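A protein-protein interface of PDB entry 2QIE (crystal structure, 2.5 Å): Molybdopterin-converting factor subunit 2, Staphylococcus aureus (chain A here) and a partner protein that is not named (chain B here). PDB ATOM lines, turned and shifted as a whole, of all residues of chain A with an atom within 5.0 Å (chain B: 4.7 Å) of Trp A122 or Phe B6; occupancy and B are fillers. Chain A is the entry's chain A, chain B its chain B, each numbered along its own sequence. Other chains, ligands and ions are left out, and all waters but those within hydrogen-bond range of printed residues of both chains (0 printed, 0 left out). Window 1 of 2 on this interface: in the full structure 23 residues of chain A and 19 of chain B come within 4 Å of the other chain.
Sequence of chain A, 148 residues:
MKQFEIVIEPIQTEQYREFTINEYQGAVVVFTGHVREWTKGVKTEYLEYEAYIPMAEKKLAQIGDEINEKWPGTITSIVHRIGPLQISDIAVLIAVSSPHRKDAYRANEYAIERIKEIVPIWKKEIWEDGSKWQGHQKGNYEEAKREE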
ATOM      1  N   GLU A  48      13.497 -31.922  38.328  1.00  0.00           N
ATOM      2  CA  GLU A  48      12.556 -30.999  37.728  1.00  0.00           C
ATOM      3  C   GLU A  48      12.542 -31.274  36.235  1.00  0.00           C
ATOM      4  O   GLU A  48      13.539 -31.053  35.555  1.00  0.00           O
ATOM      5  CB  GLU A  48      12.937 -29.546  38.034  1.00  0.00           C
ATOM      6  CG  GLU A  48      11.807 -28.564  37.789  1.00  0.00           C
ATOM      7  CD  GLU A  48      11.828 -27.367  38.751  1.00  0.00           C
ATOM      8  OE1 GLU A  48      12.127 -26.227  38.300  1.00  0.00           O
ATOM      9  OE2 GLU A  48      11.550 -27.567  39.960  1.00  0.00           O
ATOM     10  N   TYR A  49      11.427 -31.818  35.752  1.00  0.00           N
ATOM     11  CA  TYR A  49      11.236 -32.065  34.331  1.00  0.00           C
ATOM     12  C   TYR A  49      10.499 -30.892  33.700  1.00  0.00           C
ATOM     13  O   TYR A  49       9.609 -30.312  34.312  1.00  0.00           O
ATOM     14  CB  TYR A  49      10.431 -33.347  34.110  1.00  0.00           C
ATOM     15  CG  TYR A  49      11.191 -34.610  34.428  1.00  0.00           C
ATOM     16  CD1 TYR A  49      11.249 -35.097  35.725  1.00  0.00           C
ATOM     17  CD2 TYR A  49      11.854 -35.317  33.430  1.00  0.00           C
ATOM     18  CE1 TYR A  49      11.951 -36.271  36.031  1.00  0.00           C
ATOM     19  CE2 TYR A  49      12.559 -36.485  33.718  1.00  0.00           C
ATOM     20  CZ  TYR A  49      12.596 -36.954  35.022  1.00  0.00           C
ATOM     21  OH  TYR A  49      13.275 -38.095  35.319  1.00  0.00           O
ATOM     22  N   GLU A  50      10.886 -30.535  32.485  1.00  0.00           N
ATOM     23  CA  GLU A  50      10.052 -29.693  31.642  1.00  0.00           C
ATOM     24  C   GLU A  50       9.997 -30.305  30.247  1.00  0.00           C
ATOM     25  O   GLU A  50      10.743 -31.230  29.950  1.00  0.00           O
ATOM     26  CB  GLU A  50      10.536 -28.241  31.626  1.00  0.00           C
ATOM     27  CG  GLU A  50      11.800 -27.995  30.863  1.00  0.00           C
ATOM     28  CD  GLU A  50      12.275 -26.555  30.972  1.00  0.00           C
ATOM     29  OE1 GLU A  50      12.033 -25.921  32.029  1.00  0.00           O
ATOM     30  OE2 GLU A  50      12.890 -26.055  30.001  1.00  0.00           O
ATOM     31  N   ALA A  51       9.098 -29.798  29.410  1.00  0.00           N
ATOM     32  CA  ALA A  51       8.789 -30.429  28.134  1.00  0.00           C
ATOM     33  C   ALA A  51       8.193 -29.469  27.125  1.00  0.00           C
ATOM     34  O   ALA A  51       7.621 -28.439  27.479  1.00  0.00           O
ATOM     35  CB  ALA A  51       7.822 -31.577  28.353  1.00  0.00           C
ATOM     36  N   TYR A  52       8.337 -29.830  25.856  1.00  0.00           N
ATOM     37  CA  TYR A  52       7.602 -29.182  24.781  1.00  0.00           C
ATOM     38  C   TYR A  52       6.372 -30.055  24.551  1.00  0.00           C
ATOM     39  O   TYR A  52       6.390 -30.990  23.743  1.00  0.00           O
ATOM     40  CB  TYR A  52       8.487 -29.061  23.541  1.00  0.00           C
ATOM     41  CG  TYR A  52       7.903 -28.310  22.356  1.00  0.00           C
ATOM     42  CD1 TYR A  52       6.794 -27.478  22.486  1.00  0.00           C
ATOM     43  CD2 TYR A  52       8.499 -28.416  21.103  1.00  0.00           C
ATOM     44  CE1 TYR A  52       6.287 -26.793  21.394  1.00  0.00           C
ATOM     45  CE2 TYR A  52       8.004 -27.748  20.015  1.00  0.00           C
ATOM     46  CZ  TYR A  52       6.900 -26.933  20.159  1.00  0.00           C
ATOM     47  OH  TYR A  52       6.410 -26.253  19.072  1.00  0.00           O
ATOM     48  N   PRO A 120      11.033 -34.479  23.159  1.00  0.00           N
ATOM     49  CA  PRO A 120      11.465 -33.217  23.804  1.00  0.00           C
ATOM     50  C   PRO A 120      11.020 -33.062  25.265  1.00  0.00           C
ATOM     51  O   PRO A 120      10.006 -32.431  25.571  1.00  0.00           O
ATOM     52  CB  PRO A 120      10.866 -32.136  22.908  1.00  0.00           C
ATOM     53  CG  PRO A 120       9.718 -32.785  22.275  1.00  0.00           C
ATOM     54  CD  PRO A 120      10.078 -34.218  22.074  1.00  0.00           C
ATOM     55  N   ILE A 121      11.811 -33.671  26.142  1.00  0.00           N
ATOM     56  CA  ILE A 121      11.639 -33.605  27.586  1.00  0.00           C
ATOM     57  C   ILE A 121      13.029 -33.502  28.198  1.00  0.00           C
ATOM     58  O   ILE A 121      13.965 -34.142  27.726  1.00  0.00           O
ATOM     59  CB  ILE A 121      10.937 -34.873  28.135  1.00  0.00           C
ATOM     60  CG1 ILE A 121       9.502 -34.945  27.604  1.00  0.00           C
ATOM     61  CG2 ILE A 121      10.929 -34.874  29.686  1.00  0.00           C
ATOM     62  CD1 ILE A 121       8.779 -36.235  27.913  1.00  0.00           C
ATOM     63  N   TRP A 122      13.158 -32.693  29.244  1.00  0.00           N
ATOM     64  CA  TRP A 122      14.444 -32.463  29.882  1.00  0.00           C
ATOM     65  C   TRP A 122      14.327 -32.543  31.393  1.00  0.00           C
ATOM     66  O   TRP A 122      13.364 -32.037  31.961  1.00  0.00           O
ATOM     67  CB  TRP A 122      14.970 -31.097  29.484  1.00  0.00           C
ATOM     68  CG  TRP A 122      15.015 -30.931  28.019  1.00  0.00           C
ATOM     69  CD1 TRP A 122      16.031 -31.282  27.186  1.00  0.00           C
ATOM     70  CD2 TRP A 122      13.989 -30.381  27.195  1.00  0.00           C
ATOM     71  NE1 TRP A 122      15.702 -30.984  25.893  1.00  0.00           N
ATOM     72  CE2 TRP A 122      14.453 -30.426  25.868  1.00  0.00           C
ATOM     73  CE3 TRP A 122      12.727 -29.843  27.450  1.00  0.00           C
ATOM     74  CZ2 TRP A 122      13.699 -29.958  24.799  1.00  0.00           C
ATOM     75  CZ3 TRP A 122      11.974 -29.384  26.381  1.00  0.00           C
ATOM     76  CH2 TRP A 122      12.463 -29.445  25.075  1.00  0.00           C
ATOM     77  N   LYS A 123      15.309 -33.182  32.028  1.00  0.00           N
ATOM     78  CA  LYS A 123      15.359 -33.269  33.480  1.00  0.00           C
ATOM     79  C   LYS A 123      16.503 -32.429  34.024  1.00  0.00           C
ATOM     80  O   LYS A 123      17.574 -32.354  33.417  1.00  0.00           O
ATOM     81  CB  LYS A 123      15.471 -34.728  33.954  1.00  0.00           C
ATOM     82  CG  LYS A 123      16.878 -35.275  34.144  1.00  0.00           C
ATOM     83  CD  LYS A 123      16.860 -36.769  34.458  1.00  0.00           C
ATOM     84  CE  LYS A 123      16.436 -37.584  33.232  1.00  0.00           C
ATOM     85  NZ  LYS A 123      16.646 -39.047  33.371  1.00  0.00           N
ATOM     86  N   LYS A 124      16.252 -31.800  35.170  1.00  0.00           N
ATOM     87  CA  LYS A 124      17.234 -30.980  35.861  1.00  0.00           C
ATOM     88  C   LYS A 124      17.544 -31.625  37.203  1.00  0.00           C
ATOM     89  O   LYS A 124      16.676 -31.733  38.061  1.00  0.00           O
ATOM     90  CB  LYS A 124      16.684 -29.571  36.073  1.00  0.00           C
ATOM     91  CG  LYS A 124      17.709 -28.559  36.530  1.00  0.00           C
ATOM     92  CD  LYS A 124      17.083 -27.177  36.640  1.00  0.00           C
ATOM     93  CE  LYS A 124      18.135 -26.082  36.732  1.00  0.00           C
ATOM     94  NZ  LYS A 124      17.522 -24.723  36.672  1.00  0.00           N
ATOM     95  N   TRP A 133      21.108 -29.098  34.029  1.00  0.00           N
ATOM     96  CA  TRP A 133      20.301 -29.841  33.047  1.00  0.00           C
ATOM     97  C   TRP A 133      21.108 -31.009  32.459  1.00  0.00           C
ATOM     98  O   TRP A 133      22.280 -30.855  32.137  1.00  0.00           O
ATOM     99  CB  TRP A 133      19.812 -28.933  31.914  1.00  0.00           C
ATOM    100  CG  TRP A 133      18.837 -27.889  32.350  1.00  0.00           C
ATOM    101  CD1 TRP A 133      19.111 -26.585  32.616  1.00  0.00           C
ATOM    102  CD2 TRP A 133      17.429 -28.060  32.576  1.00  0.00           C
ATOM    103  NE1 TRP A 133      17.969 -25.931  32.994  1.00  0.00           N
ATOM    104  CE2 TRP A 133      16.920 -26.812  32.982  1.00  0.00           C
ATOM    105  CE3 TRP A 133      16.554 -29.151  32.490  1.00  0.00           C
ATOM    106  CZ2 TRP A 133      15.568 -26.612  33.287  1.00  0.00           C
ATOM    107  CZ3 TRP A 133      15.200 -28.955  32.800  1.00  0.00           C
ATOM    108  CH2 TRP A 133      14.728 -27.693  33.194  1.00  0.00           C
ATOM    109  N   LEU B   4      10.662 -20.599  20.637  1.00  0.00           N
ATOM    110  CA  LEU B   4      10.512 -21.186  21.985  1.00  0.00           C
ATOM    111  C   LEU B   4      11.855 -21.711  22.502  1.00  0.00           C
ATOM    112  O   LEU B   4      12.621 -22.322  21.750  1.00  0.00           O
ATOM    113  CB  LEU B   4       9.500 -22.332  21.982  1.00  0.00           C
ATOM    114  CG  LEU B   4       8.086 -22.039  21.491  1.00  0.00           C
ATOM    115  CD1 LEU B   4       7.241 -23.308  21.539  1.00  0.00           C
ATOM    116  CD2 LEU B   4       7.428 -20.937  22.311  1.00  0.00           C
ATOM    117  N   TYR B   5      12.122 -21.474  23.784  1.00  0.00           N
ATOM    118  CA  TYR B   5      13.375 -21.890  24.429  1.00  0.00           C
ATOM    119  C   TYR B   5      13.122 -22.796  25.635  1.00  0.00           C
ATOM    120  O   TYR B   5      12.177 -22.609  26.374  1.00  0.00           O
ATOM    121  CB  TYR B   5      14.198 -20.667  24.860  1.00  0.00           C
ATOM    122  CG  TYR B   5      14.416 -19.617  23.781  1.00  0.00           C
ATOM    123  CD1 TYR B   5      13.784 -18.376  23.855  1.00  0.00           C
ATOM    124  CD2 TYR B   5      15.253 -19.860  22.699  1.00  0.00           C
ATOM    125  CE1 TYR B   5      13.971 -17.403  22.876  1.00  0.00           C
ATOM    126  CE2 TYR B   5      15.454 -18.894  21.717  1.00  0.00           C
ATOM    127  CZ  TYR B   5      14.807 -17.667  21.811  1.00  0.00           C
ATOM    128  OH  TYR B   5      14.990 -16.702  20.839  1.00  0.00           O
ATOM    129  N   PHE B   6      13.985 -23.775  25.835  1.00  0.00           N
ATOM    130  CA  PHE B   6      13.792 -24.782  26.874  1.00  0.00           C
ATOM    131  C   PHE B   6      15.111 -25.141  27.554  1.00  0.00           C
ATOM    132  O   PHE B   6      16.199 -24.964  26.998  1.00  0.00           O
ATOM    133  CB  PHE B   6      13.202 -26.077  26.277  1.00  0.00           C
ATOM    134  CG  PHE B   6      11.862 -25.901  25.599  1.00  0.00           C
ATOM    135  CD1 PHE B   6      11.785 -25.686  24.227  1.00  0.00           C
ATOM    136  CD2 PHE B   6      10.683 -25.970  26.325  1.00  0.00           C
ATOM    137  CE1 PHE B   6      10.553 -25.535  23.599  1.00  0.00           C
ATOM    138  CE2 PHE B   6       9.452 -25.819  25.703  1.00  0.00           C
ATOM    139  CZ  PHE B   6       9.386 -25.602  24.343  1.00  0.00           C
ATOM    140  N   ALA B   7      14.986 -25.691  28.750  1.00  0.00           N
ATOM    141  CA  ALA B   7      16.108 -26.201  29.516  1.00  0.00           C
ATOM    142  C   ALA B   7      17.179 -25.133  29.699  1.00  0.00           C
ATOM    143  O   ALA B   7      16.871 -24.044  30.173  1.00  0.00           O
ATOM    144  CB  ALA B   7      16.662 -27.484  28.883  1.00  0.00           C
ATOM    145  N   GLU B   8      18.418 -25.426  29.323  1.00  0.00           N
ATOM    146  CA  GLU B   8      19.539 -24.565  29.670  1.00  0.00           C
ATOM    147  C   GLU B   8      19.516 -23.236  28.932  1.00  0.00           C
ATOM    148  O   GLU B   8      20.012 -22.238  29.447  1.00  0.00           O
ATOM    149  CB  GLU B   8      20.845 -25.290  29.387  1.00  0.00           C
ATOM    150  CG  GLU B   8      22.067 -24.650  30.016  1.00  0.00           C
ATOM    151  CD  GLU B   8      23.294 -25.528  29.894  1.00  0.00           C
ATOM    152  OE1 GLU B   8      23.147 -26.744  29.632  1.00  0.00           O
ATOM    153  OE2 GLU B   8      24.413 -25.005  30.064  1.00  0.00           O
ATOM    154  N   ILE B   9      18.946 -23.239  27.729  1.00  0.00           N
ATOM    155  CA  ILE B   9      18.897 -22.050  26.880  1.00  0.00           C
ATOM    156  C   ILE B   9      17.869 -21.059  27.412  1.00  0.00           C
ATOM    157  O   ILE B   9      18.129 -19.847  27.461  1.00  0.00           O
ATOM    158  CB  ILE B   9      18.607 -22.428  25.403  1.00  0.00           C
ATOM    159  CG1 ILE B   9      19.864 -23.053  24.786  1.00  0.00           C
ATOM    160  CG2 ILE B   9      18.204 -21.203  24.575  1.00  0.00           C
ATOM    161  CD1 ILE B   9      19.618 -23.791  23.525  1.00  0.00           C
ATOM    162  N   LYS B  10      16.708 -21.581  27.804  1.00  0.00           N
ATOM    163  CA  LYS B  10      15.695 -20.793  28.525  1.00  0.00           C
ATOM    164  C   LYS B  10      16.351 -20.092  29.718  1.00  0.00           C
ATOM    165  O   LYS B  10      16.129 -18.904  29.953  1.00  0.00           O
ATOM    166  CB  LYS B  10      14.576 -21.722  29.014  1.00  0.00           C
ATOM    167  CG  LYS B  10      13.292 -21.053  29.491  1.00  0.00           C
ATOM    168  CD  LYS B  10      12.383 -22.102  30.157  1.00  0.00           C
ATOM    169  CE  LYS B  10      11.017 -21.553  30.518  1.00  0.00           C
ATOM    170  NZ  LYS B  10      10.278 -22.410  31.501  1.00  0.00           N
ATOM    171  N   ALA B  69      11.441 -24.017  17.548  1.00  0.00           N
ATOM    172  CA  ALA B  69      11.796 -24.425  18.898  1.00  0.00           C
ATOM    173  C   ALA B  69      13.209 -24.947  18.967  1.00  0.00           C
ATOM    174  O   ALA B  69      13.580 -25.835  18.199  1.00  0.00           O
ATOM    175  CB  ALA B  69      10.839 -25.472  19.381  1.00  0.00           C
ATOM    176  N   LEU B  70      13.992 -24.395  19.890  1.00  0.00           N
ATOM    177  CA  LEU B  70      15.355 -24.853  20.096  1.00  0.00           C
ATOM    178  C   LEU B  70      15.315 -26.022  21.069  1.00  0.00           C
ATOM    179  O   LEU B  70      14.938 -25.857  22.211  1.00  0.00           O
ATOM    180  CB  LEU B  70      16.232 -23.731  20.643  1.00  0.00           C
ATOM    181  CG  LEU B  70      16.171 -22.361  19.973  1.00  0.00           C
ATOM    182  CD1 LEU B  70      17.459 -21.621  20.281  1.00  0.00           C
ATOM    183  CD2 LEU B  70      15.951 -22.448  18.469  1.00  0.00           C
ATOM    184  N   ILE B  71      15.685 -27.198  20.593  1.00  0.00           N
ATOM    185  CA  ILE B  71      15.606 -28.439  21.355  1.00  0.00           C
ATOM    186  C   ILE B  71      17.000 -28.898  21.766  1.00  0.00           C
ATOM    187  O   ILE B  71      17.680 -29.529  20.976  1.00  0.00           O
ATOM    188  CB  ILE B  71      14.977 -29.573  20.478  1.00  0.00           C
ATOM    189  CG1 ILE B  71      13.607 -29.144  19.935  1.00  0.00           C
ATOM    190  CG2 ILE B  71      14.857 -30.866  21.247  1.00  0.00           C
ATOM    191  CD1 ILE B  71      12.619 -28.710  20.990  1.00  0.00           C
ATOM    192  N   PRO B  72      17.429 -28.597  23.006  1.00  0.00           N
ATOM    193  CA  PRO B  72      18.731 -29.087  23.464  1.00  0.00           C
ATOM    194  C   PRO B  72      18.705 -30.603  23.660  1.00  0.00           C
ATOM    195  O   PRO B  72      17.624 -31.184  23.669  1.00  0.00           O
ATOM    196  CB  PRO B  72      18.926 -28.383  24.815  1.00  0.00           C
ATOM    197  CG  PRO B  72      17.890 -27.355  24.885  1.00  0.00           C
ATOM    198  CD  PRO B  72      16.757 -27.824  24.053  1.00  0.00           C
ATOM    199  N   PRO B  73      19.884 -31.242  23.821  1.00  0.00           N
ATOM    200  CA  PRO B  73      19.936 -32.699  23.991  1.00  0.00           C
ATOM    201  C   PRO B  73      18.931 -33.209  25.028  1.00  0.00           C
ATOM    202  O   PRO B  73      18.998 -32.850  26.205  1.00  0.00           O
ATOM    203  CB  PRO B  73      21.385 -32.948  24.440  1.00  0.00           C
ATOM    204  CG  PRO B  73      22.140 -31.871  23.790  1.00  0.00           C
ATOM    205  CD  PRO B  73      21.234 -30.655  23.867  1.00  0.00           C
ATOM    206  N   VAL B  74      17.996 -34.019  24.563  1.00  0.00           N
ATOM    207  CA  VAL B  74      16.909 -34.510  25.398  1.00  0.00           C
ATOM    208  C   VAL B  74      17.388 -35.415  26.536  1.00  0.00           C
ATOM    209  O   VAL B  74      18.434 -36.084  26.443  1.00  0.00           O
ATOM    210  CB  VAL B  74      15.841 -35.248  24.574  1.00  0.00           C
ATOM    211  CG1 VAL B  74      15.194 -34.277  23.571  1.00  0.00           C
ATOM    212  CG2 VAL B  74      16.422 -36.467  23.875  1.00  0.00           C
ATOM    213  N   SER B  75      16.602 -35.418  27.609  1.00  0.00           N
ATOM    214  CA  SER B  75      16.919 -36.189  28.802  1.00  0.00           C
ATOM    215  C   SER B  75      15.627 -36.586  29.501  1.00  0.00           C
ATOM    216  O   SER B  75      15.433 -36.319  30.686  1.00  0.00           O
ATOM    217  CB  SER B  75      17.824 -35.370  29.732  1.00  0.00           C
ATOM    218  OG  SER B  75      17.278 -34.090  29.991  1.00  0.00           O
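OE2 of Glu A50 sits at hydrogen-bond distance from N of Ala B7, 2.5 Å away. OE1 of Glu A50 lies within salt-bridge range of NZ of Lys B10, at 3.96 Å. The backbone carbonyl oxygen of Ile A121 sits at hydrogen-bond distance from the backbone NH of Ser B75. NE1 of Trp A122 sits at hydrogen-bond distance from O of Pro B72, at 2.9 Å. The backbone NH (N) of Lys A123 sits at hydrogen-bond distance from the side-chain hydroxyl (OG) of Ser B75 (3.0 Å).
The backbone carbonyl oxygen (O) of Glu A50 sits at hydrogen-bond distance from the backbone NH (N) of Trp A122. The backbone carbonyl oxygen of Pro A120 is in hydrogen-bond range of the backbone NH of Tyr A52. O of Leu B4 sits at hydrogen-bond distance from N of Leu B70, 3.1 Å away.
Glu A50 touches Phe B6. CZ of Phe B6 touches CB of Tyr A52, 3.7 Å away. CE2 of Tyr A52 touches CB of Ala B69 (3.7 Å). CG1 of Val B74 touches CA of Pro A120 (3.9 Å). Trp A122 touches Phe B6 (CZ3 to CB, 3.5 Å). CB of Ala B7 touches CG of Trp A122 (3.9 Å). Trp A122 touches Pro B73 (CD1 to O, 3.5 Å). Trp A122 touches Ser B75. Trp A133 touches Ala B7. Trp A133 touches Glu B8.
Of the printed residues of chain B, Ala A51 touches Phe B6. Of chain B, only Phe B6 (3.5 Å), Ala B7 (3.9 Å), Ile B71 (3.8 Å), Pro B72 (2.9 Å), Pro B73 (3.5 Å), Val B74 (3.8 Å) and Ser B75 (3.3 Å) come within 4 Å of Trp A122. Phe B6 touches just these residues of chain A: Glu A50, Ala A51, Tyr A52 and Trp A122. Of the printed residues of chain A, Pro B72 touches Trp A122 (2.9 Å). The nearest printed residue of chain B that does not touch Trp A122 is Leu B70 (5.0 Å). The nearest printed residue of chain A that does not touch Pro B73 is Ile A121 (5.4 Å).
Hydrophobic or aromatic side chains of chain B that line the printed part of chain A: Leu B4, Phe B6, Ala B7, Ala B69, Ile B71, Pro B72 and Val B74.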
